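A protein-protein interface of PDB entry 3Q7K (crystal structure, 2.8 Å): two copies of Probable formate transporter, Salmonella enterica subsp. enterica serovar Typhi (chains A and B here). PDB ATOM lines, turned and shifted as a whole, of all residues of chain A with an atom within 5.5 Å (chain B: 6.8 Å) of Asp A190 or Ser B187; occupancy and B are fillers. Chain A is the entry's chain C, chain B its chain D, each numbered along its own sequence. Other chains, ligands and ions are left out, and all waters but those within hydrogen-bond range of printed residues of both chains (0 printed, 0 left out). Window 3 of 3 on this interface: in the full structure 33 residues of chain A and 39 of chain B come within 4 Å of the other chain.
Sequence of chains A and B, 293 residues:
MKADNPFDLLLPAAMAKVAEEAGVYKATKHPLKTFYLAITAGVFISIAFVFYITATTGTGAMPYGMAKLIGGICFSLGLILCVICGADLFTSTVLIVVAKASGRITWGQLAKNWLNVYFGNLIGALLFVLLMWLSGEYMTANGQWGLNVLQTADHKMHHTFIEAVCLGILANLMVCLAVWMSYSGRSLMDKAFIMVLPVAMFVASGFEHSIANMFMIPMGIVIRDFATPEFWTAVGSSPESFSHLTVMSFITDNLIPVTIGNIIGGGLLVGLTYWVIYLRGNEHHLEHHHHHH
Of chain A, only Asp A190 comes within 4 Å of Ser B187.
Printed residues of chain A within 4 Å of Leu B188: Ser A184 (3.6 Å), Gly A185 (3.7 Å), Asp A190 (3.2 Å) and Ile A194 (3.7 Å).
Of the printed residues of chain A, Ala B192 touches Ile A194 (3.7 Å).
Arg B186 touches none of the printed residues of chain A.
Arg A186 touches none of the printed residues of chain B.
The nearest residue of chain A that does not touch Ser B187 is Arg A186 (4.3 Å).
The nearest printed residue of chain A that does not touch Leu B188 is Lys A191 (4.8 Å).
Ser A184 touches Leu B188, but with the chains exchanged Leu A188 does not touch Ser B184 (17.4 Å).
Gly A185 touches Leu B188, but with the chains exchanged Leu A188 does not touch Gly B185 (15.2 Å).
Met A189 touches its own counterpart, Met B189.
Asp A190 touches Ser B187, but with the chains exchanged Ser A187 does not touch Asp B190 (8.0 Å).
Hydrophobic or aromatic side chains of chain B that line the printed part of chain A: Leu B188, Met B189 and Ala B192.
Among the printed residues, no Asp or Glu carboxylate lies within 4 Å of a Lys or Arg side-chain nitrogen of the other chain.
N of Arg A186 is in hydrogen-bond range of OD2 of Asp A190.
OG of Ser A187 sits close to OD2 of Asp A190.
OG of Ser B187 is in hydrogen-bond range of N of Asp B190 (3.1 Å).
The side-chain carboxylate of Asp A190 lies close to the backbone NH of Leu B188, at 3.3 Å.
The backbone NH (N) of Met B189 lies within hydrogen-bond range of the side-chain carboxylate (OD1) of Asp A190 (2.7 Å).
O of Met A189 lies close to SD of Met B189 (3.6 Å).
Among the printed residues, pairs that only touch across the chains: Ser A184 with Leu B188 (3.6 Å), Gly A185 with Leu B188 (3.7 Å), Asp A190 with Ser B187 (3.7 Å), Phe A193 with Met B189 (3.96 Å), Ile A194 with Leu B188 (3.7 Å) and Ile A194 with Ala B192 (3.7 Å).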
ATOM      1  N   SER A 184      15.408 -23.042 -16.585  1.00  0.00           N
ATOM      2  CA  SER A 184      14.535 -23.756 -17.546  1.00  0.00           C
ATOM      3  C   SER A 184      13.301 -24.327 -16.841  1.00  0.00           C
ATOM      4  O   SER A 184      12.403 -24.879 -17.477  1.00  0.00           O
ATOM      5  CB  SER A 184      15.258 -24.906 -18.255  1.00  0.00           C
ATOM      6  OG  SER A 184      16.314 -24.469 -19.063  1.00  0.00           O
ATOM      7  N   GLY A 185      13.264 -24.186 -15.534  1.00  0.00           N
ATOM      8  CA  GLY A 185      12.200 -24.753 -14.757  1.00  0.00           C
ATOM      9  C   GLY A 185      10.875 -24.117 -15.024  1.00  0.00           C
ATOM     10  O   GLY A 185      10.750 -22.919 -15.007  1.00  0.00           O
ATOM     11  N   ARG A 186       9.892 -24.958 -15.264  1.00  0.00           N
ATOM     12  CA  ARG A 186       8.533 -24.551 -15.503  1.00  0.00           C
ATOM     13  C   ARG A 186       7.683 -24.699 -14.273  1.00  0.00           C
ATOM     14  O   ARG A 186       6.747 -23.963 -14.093  1.00  0.00           O
ATOM     15  CB  ARG A 186       7.925 -25.423 -16.569  1.00  0.00           C
ATOM     16  CG  ARG A 186       8.597 -25.384 -17.882  1.00  0.00           C
ATOM     17  CD  ARG A 186       7.757 -26.097 -18.917  1.00  0.00           C
ATOM     18  NE  ARG A 186       7.410 -25.226 -20.028  1.00  0.00           N
ATOM     19  CZ  ARG A 186       6.212 -24.691 -20.226  1.00  0.00           C
ATOM     20  NH1 ARG A 186       5.206 -24.931 -19.398  1.00  0.00           N
ATOM     21  NH2 ARG A 186       6.021 -23.902 -21.260  1.00  0.00           N
ATOM     22  N   SER A 187       7.996 -25.666 -13.435  1.00  0.00           N
ATOM     23  CA  SER A 187       7.201 -25.910 -12.266  1.00  0.00           C
ATOM     24  C   SER A 187       8.036 -25.844 -11.042  1.00  0.00           C
ATOM     25  O   SER A 187       9.218 -25.689 -11.133  1.00  0.00           O
ATOM     26  CB  SER A 187       6.620 -27.286 -12.346  1.00  0.00           C
ATOM     27  OG  SER A 187       7.454 -28.109 -13.098  1.00  0.00           O
ATOM     28  N   LEU A 188       7.412 -25.976  -9.885  1.00  0.00           N
ATOM     29  CA  LEU A 188       8.168 -26.242  -8.649  1.00  0.00           C
ATOM     30  C   LEU A 188       8.937 -27.562  -8.782  1.00  0.00           C
ATOM     31  O   LEU A 188      10.128 -27.617  -8.545  1.00  0.00           O
ATOM     32  CB  LEU A 188       7.201 -26.360  -7.470  1.00  0.00           C
ATOM     33  CG  LEU A 188       7.694 -26.086  -6.069  1.00  0.00           C
ATOM     34  CD1 LEU A 188       8.320 -24.711  -6.127  1.00  0.00           C
ATOM     35  CD2 LEU A 188       6.514 -26.116  -5.090  1.00  0.00           C
ATOM     36  N   MET A 189       8.231 -28.620  -9.169  1.00  0.00           N
ATOM     37  CA  MET A 189       8.836 -29.913  -9.510  1.00  0.00           C
ATOM     38  C   MET A 189      10.101 -29.795 -10.361  1.00  0.00           C
ATOM     39  O   MET A 189      11.103 -30.464 -10.093  1.00  0.00           O
ATOM     40  CB  MET A 189       7.828 -30.770 -10.265  1.00  0.00           C
ATOM     41  CG  MET A 189       7.993 -32.228 -10.053  1.00  0.00           C
ATOM     42  SD  MET A 189       7.732 -32.511  -8.300  1.00  0.00           S
ATOM     43  CE  MET A 189       9.023 -33.741  -8.007  1.00  0.00           C
ATOM     44  N   ASP A 190      10.022 -28.945 -11.385  1.00  0.00           N
ATOM     45  CA  ASP A 190      11.104 -28.730 -12.320  1.00  0.00           C
ATOM     46  C   ASP A 190      12.275 -28.079 -11.656  1.00  0.00           C
ATOM     47  O   ASP A 190      13.369 -28.593 -11.715  1.00  0.00           O
ATOM     48  CB  ASP A 190      10.639 -27.836 -13.455  1.00  0.00           C
ATOM     49  CG  ASP A 190      10.082 -28.608 -14.619  1.00  0.00           C
ATOM     50  OD1 ASP A 190      10.232 -29.854 -14.644  1.00  0.00           O
ATOM     51  OD2 ASP A 190       9.510 -27.957 -15.516  1.00  0.00           O
ATOM     52  N   LYS A 191      12.036 -26.946 -11.015  1.00  0.00           N
ATOM     53  CA  LYS A 191      13.120 -26.158 -10.459  1.00  0.00           C
ATOM     54  C   LYS A 191      13.875 -26.900  -9.367  1.00  0.00           C
ATOM     55  O   LYS A 191      15.100 -26.844  -9.322  1.00  0.00           O
ATOM     56  CB  LYS A 191      12.599 -24.823  -9.959  1.00  0.00           C
ATOM     57  CG  LYS A 191      12.043 -23.919 -11.076  1.00  0.00           C
ATOM     58  CD  LYS A 191      11.431 -22.622 -10.518  1.00  0.00           C
ATOM     59  CE  LYS A 191      10.973 -21.670 -11.636  1.00  0.00           C
ATOM     60  NZ  LYS A 191       9.726 -20.913 -11.276  1.00  0.00           N
ATOM     61  N   ALA A 192      13.151 -27.622  -8.515  1.00  0.00           N
ATOM     62  CA  ALA A 192      13.747 -28.271  -7.345  1.00  0.00           C
ATOM     63  C   ALA A 192      14.500 -29.517  -7.738  1.00  0.00           C
ATOM     64  O   ALA A 192      15.676 -29.661  -7.447  1.00  0.00           O
ATOM     65  CB  ALA A 192      12.692 -28.610  -6.318  1.00  0.00           C
ATOM     66  N   PHE A 193      13.824 -30.420  -8.414  1.00  0.00           N
ATOM     67  CA  PHE A 193      14.405 -31.715  -8.721  1.00  0.00           C
ATOM     68  C   PHE A 193      15.529 -31.731  -9.747  1.00  0.00           C
ATOM     69  O   PHE A 193      16.330 -32.609  -9.724  1.00  0.00           O
ATOM     70  CB  PHE A 193      13.289 -32.743  -9.013  1.00  0.00           C
ATOM     71  CG  PHE A 193      12.656 -33.340  -7.735  1.00  0.00           C
ATOM     72  CD1 PHE A 193      12.572 -34.746  -7.572  1.00  0.00           C
ATOM     73  CD2 PHE A 193      12.204 -32.496  -6.675  1.00  0.00           C
ATOM     74  CE1 PHE A 193      12.029 -35.329  -6.398  1.00  0.00           C
ATOM     75  CE2 PHE A 193      11.669 -33.038  -5.492  1.00  0.00           C
ATOM     76  CZ  PHE A 193      11.570 -34.483  -5.355  1.00  0.00           C
ATOM     77  N   ILE A 194      15.629 -30.732 -10.607  1.00  0.00           N
ATOM     78  CA  ILE A 194      16.723 -30.650 -11.590  1.00  0.00           C
ATOM     79  C   ILE A 194      18.040 -30.372 -10.867  1.00  0.00           C
ATOM     80  O   ILE A 194      19.105 -30.657 -11.376  1.00  0.00           O
ATOM     81  CB  ILE A 194      16.459 -29.582 -12.732  1.00  0.00           C
ATOM     82  CG1 ILE A 194      17.372 -29.784 -13.940  1.00  0.00           C
ATOM     83  CG2 ILE A 194      16.597 -28.195 -12.239  1.00  0.00           C
ATOM     84  CD1 ILE A 194      17.092 -31.084 -14.630  1.00  0.00           C
ATOM     85  N   MET A 195      17.945 -29.831  -9.666  1.00  0.00           N
ATOM     86  CA  MET A 195      19.102 -29.551  -8.857  1.00  0.00           C
ATOM     87  C   MET A 195      19.619 -30.740  -8.007  1.00  0.00           C
ATOM     88  O   MET A 195      20.781 -30.710  -7.571  1.00  0.00           O
ATOM     89  CB  MET A 195      18.827 -28.339  -8.004  1.00  0.00           C
ATOM     90  CG  MET A 195      18.459 -27.162  -8.859  1.00  0.00           C
ATOM     91  SD  MET A 195      18.634 -25.596  -8.010  1.00  0.00           S
ATOM     92  CE  MET A 195      17.478 -25.796  -6.663  1.00  0.00           C
ATOM     93  N   GLU B  21      15.341 -22.992 -23.507  1.00  0.00           N
ATOM     94  CA  GLU B  21      15.368 -24.234 -24.307  1.00  0.00           C
ATOM     95  C   GLU B  21      15.424 -24.024 -25.820  1.00  0.00           C
ATOM     96  O   GLU B  21      15.891 -24.905 -26.544  1.00  0.00           O
ATOM     97  CB  GLU B  21      14.291 -25.245 -23.887  1.00  0.00           C
ATOM     98  CG  GLU B  21      14.603 -26.756 -24.309  1.00  0.00           C
ATOM     99  CD  GLU B  21      15.624 -27.577 -23.412  1.00  0.00           C
ATOM    100  OE1 GLU B  21      16.571 -28.176 -24.008  1.00  0.00           O
ATOM    101  OE2 GLU B  21      15.459 -27.662 -22.154  1.00  0.00           O
ATOM    102  N   ILE B  84      19.769 -30.426 -21.386  1.00  0.00           N
ATOM    103  CA  ILE B  84      19.138 -29.230 -20.835  1.00  0.00           C
ATOM    104  C   ILE B  84      19.959 -27.997 -21.091  1.00  0.00           C
ATOM    105  O   ILE B  84      19.373 -26.944 -21.228  1.00  0.00           O
ATOM    106  CB  ILE B  84      18.898 -29.317 -19.329  1.00  0.00           C
ATOM    107  CG1 ILE B  84      18.077 -30.556 -18.972  1.00  0.00           C
ATOM    108  CG2 ILE B  84      18.289 -28.003 -18.773  1.00  0.00           C
ATOM    109  CD1 ILE B  84      16.781 -30.660 -19.722  1.00  0.00           C
ATOM    110  N   SER B 182      13.863 -37.676 -25.165  1.00  0.00           N
ATOM    111  CA  SER B 182      13.905 -36.359 -24.542  1.00  0.00           C
ATOM    112  C   SER B 182      13.210 -35.291 -25.378  1.00  0.00           C
ATOM    113  O   SER B 182      12.682 -34.355 -24.820  1.00  0.00           O
ATOM    114  CB  SER B 182      15.347 -35.957 -24.219  1.00  0.00           C
ATOM    115  OG  SER B 182      15.347 -34.919 -23.238  1.00  0.00           O
ATOM    116  N   SER B 184      10.229 -35.634 -27.160  1.00  0.00           N
ATOM    117  CA  SER B 184       8.837 -35.634 -26.735  1.00  0.00           C
ATOM    118  C   SER B 184       8.667 -34.825 -25.457  1.00  0.00           C
ATOM    119  O   SER B 184       7.536 -34.438 -25.103  1.00  0.00           O
ATOM    120  CB  SER B 184       8.403 -37.057 -26.424  1.00  0.00           C
ATOM    121  OG  SER B 184       8.815 -37.936 -27.449  1.00  0.00           O
ATOM    122  N   GLY B 185       9.776 -34.578 -24.758  1.00  0.00           N
ATOM    123  CA  GLY B 185       9.721 -33.956 -23.451  1.00  0.00           C
ATOM    124  C   GLY B 185       9.219 -32.543 -23.483  1.00  0.00           C
ATOM    125  O   GLY B 185       9.675 -31.751 -24.270  1.00  0.00           O
ATOM    126  N   ARG B 186       8.268 -32.230 -22.633  1.00  0.00           N
ATOM    127  CA  ARG B 186       7.730 -30.882 -22.599  1.00  0.00           C
ATOM    128  C   ARG B 186       8.363 -30.146 -21.409  1.00  0.00           C
ATOM    129  O   ARG B 186       8.854 -29.052 -21.579  1.00  0.00           O
ATOM    130  CB  ARG B 186       6.160 -30.846 -22.677  1.00  0.00           C
ATOM    131  CG  ARG B 186       5.310 -32.250 -22.387  1.00  0.00           C
ATOM    132  CD  ARG B 186       3.784 -32.147 -22.918  1.00  0.00           C
ATOM    133  NE  ARG B 186       3.484 -30.761 -22.599  1.00  0.00           N
ATOM    134  CZ  ARG B 186       2.545 -29.910 -22.991  1.00  0.00           C
ATOM    135  NH1 ARG B 186       2.674 -28.692 -22.477  1.00  0.00           N
ATOM    136  NH2 ARG B 186       1.533 -30.194 -23.812  1.00  0.00           N
ATOM    137  N   SER B 187       8.409 -30.778 -20.231  1.00  0.00           N
ATOM    138  CA  SER B 187       8.995 -30.174 -19.021  1.00  0.00           C
ATOM    139  C   SER B 187      10.464 -30.541 -18.806  1.00  0.00           C
ATOM    140  O   SER B 187      11.027 -31.365 -19.526  1.00  0.00           O
ATOM    141  CB  SER B 187       8.189 -30.522 -17.758  1.00  0.00           C
ATOM    142  OG  SER B 187       7.985 -31.913 -17.579  1.00  0.00           O
ATOM    143  N   LEU B 188      11.074 -29.906 -17.810  1.00  0.00           N
ATOM    144  CA  LEU B 188      12.433 -30.190 -17.410  1.00  0.00           C
ATOM    145  C   LEU B 188      12.429 -31.573 -16.795  1.00  0.00           C
ATOM    146  O   LEU B 188      13.375 -32.339 -16.925  1.00  0.00           O
ATOM    147  CB  LEU B 188      12.857 -29.178 -16.356  1.00  0.00           C
ATOM    148  CG  LEU B 188      14.316 -28.808 -16.147  1.00  0.00           C
ATOM    149  CD1 LEU B 188      14.904 -28.398 -17.472  1.00  0.00           C
ATOM    150  CD2 LEU B 188      14.418 -27.678 -15.171  1.00  0.00           C
ATOM    151  N   MET B 189      11.326 -31.886 -16.128  1.00  0.00           N
ATOM    152  CA  MET B 189      11.083 -33.196 -15.533  1.00  0.00           C
ATOM    153  C   MET B 189      11.004 -34.280 -16.596  1.00  0.00           C
ATOM    154  O   MET B 189      11.619 -35.324 -16.474  1.00  0.00           O
ATOM    155  CB  MET B 189       9.759 -33.124 -14.786  1.00  0.00           C
ATOM    156  CG  MET B 189       9.659 -33.981 -13.551  1.00  0.00           C
ATOM    157  SD  MET B 189      10.712 -33.361 -12.242  1.00  0.00           S
ATOM    158  CE  MET B 189      11.359 -34.941 -11.684  1.00  0.00           C
ATOM    159  N   ASP B 190      10.239 -34.026 -17.648  1.00  0.00           N
ATOM    160  CA  ASP B 190      10.131 -34.937 -18.774  1.00  0.00           C
ATOM    161  C   ASP B 190      11.492 -35.191 -19.414  1.00  0.00           C
ATOM    162  O   ASP B 190      11.870 -36.330 -19.694  1.00  0.00           O
ATOM    163  CB  ASP B 190       9.249 -34.317 -19.859  1.00  0.00           C
ATOM    164  CG  ASP B 190       7.756 -34.433 -19.587  1.00  0.00           C
ATOM    165  OD1 ASP B 190       7.339 -35.179 -18.664  1.00  0.00           O
ATOM    166  OD2 ASP B 190       6.976 -33.769 -20.335  1.00  0.00           O
ATOM    167  N   LYS B 191      12.207 -34.103 -19.687  1.00  0.00           N
ATOM    168  CA  LYS B 191      13.416 -34.199 -20.468  1.00  0.00           C
ATOM    169  C   LYS B 191      14.544 -34.866 -19.659  1.00  0.00           C
ATOM    170  O   LYS B 191      15.336 -35.687 -20.184  1.00  0.00           O
ATOM    171  CB  LYS B 191      13.842 -32.827 -20.997  1.00  0.00           C
ATOM    172  CG  LYS B 191      12.900 -32.206 -22.001  1.00  0.00           C
ATOM    173  CD  LYS B 191      13.572 -31.044 -22.721  1.00  0.00           C
ATOM    174  CE  LYS B 191      12.610 -30.279 -23.657  1.00  0.00           C
ATOM    175  NZ  LYS B 191      12.201 -28.874 -23.122  1.00  0.00           N
ATOM    176  N   ALA B 192      14.616 -34.524 -18.377  1.00  0.00           N
ATOM    177  CA  ALA B 192      15.720 -35.036 -17.571  1.00  0.00           C
ATOM    178  C   ALA B 192      15.450 -36.475 -17.223  1.00  0.00           C
ATOM    179  O   ALA B 192      16.268 -37.348 -17.515  1.00  0.00           O
ATOM    180  CB  ALA B 192      15.958 -34.198 -16.312  1.00  0.00           C
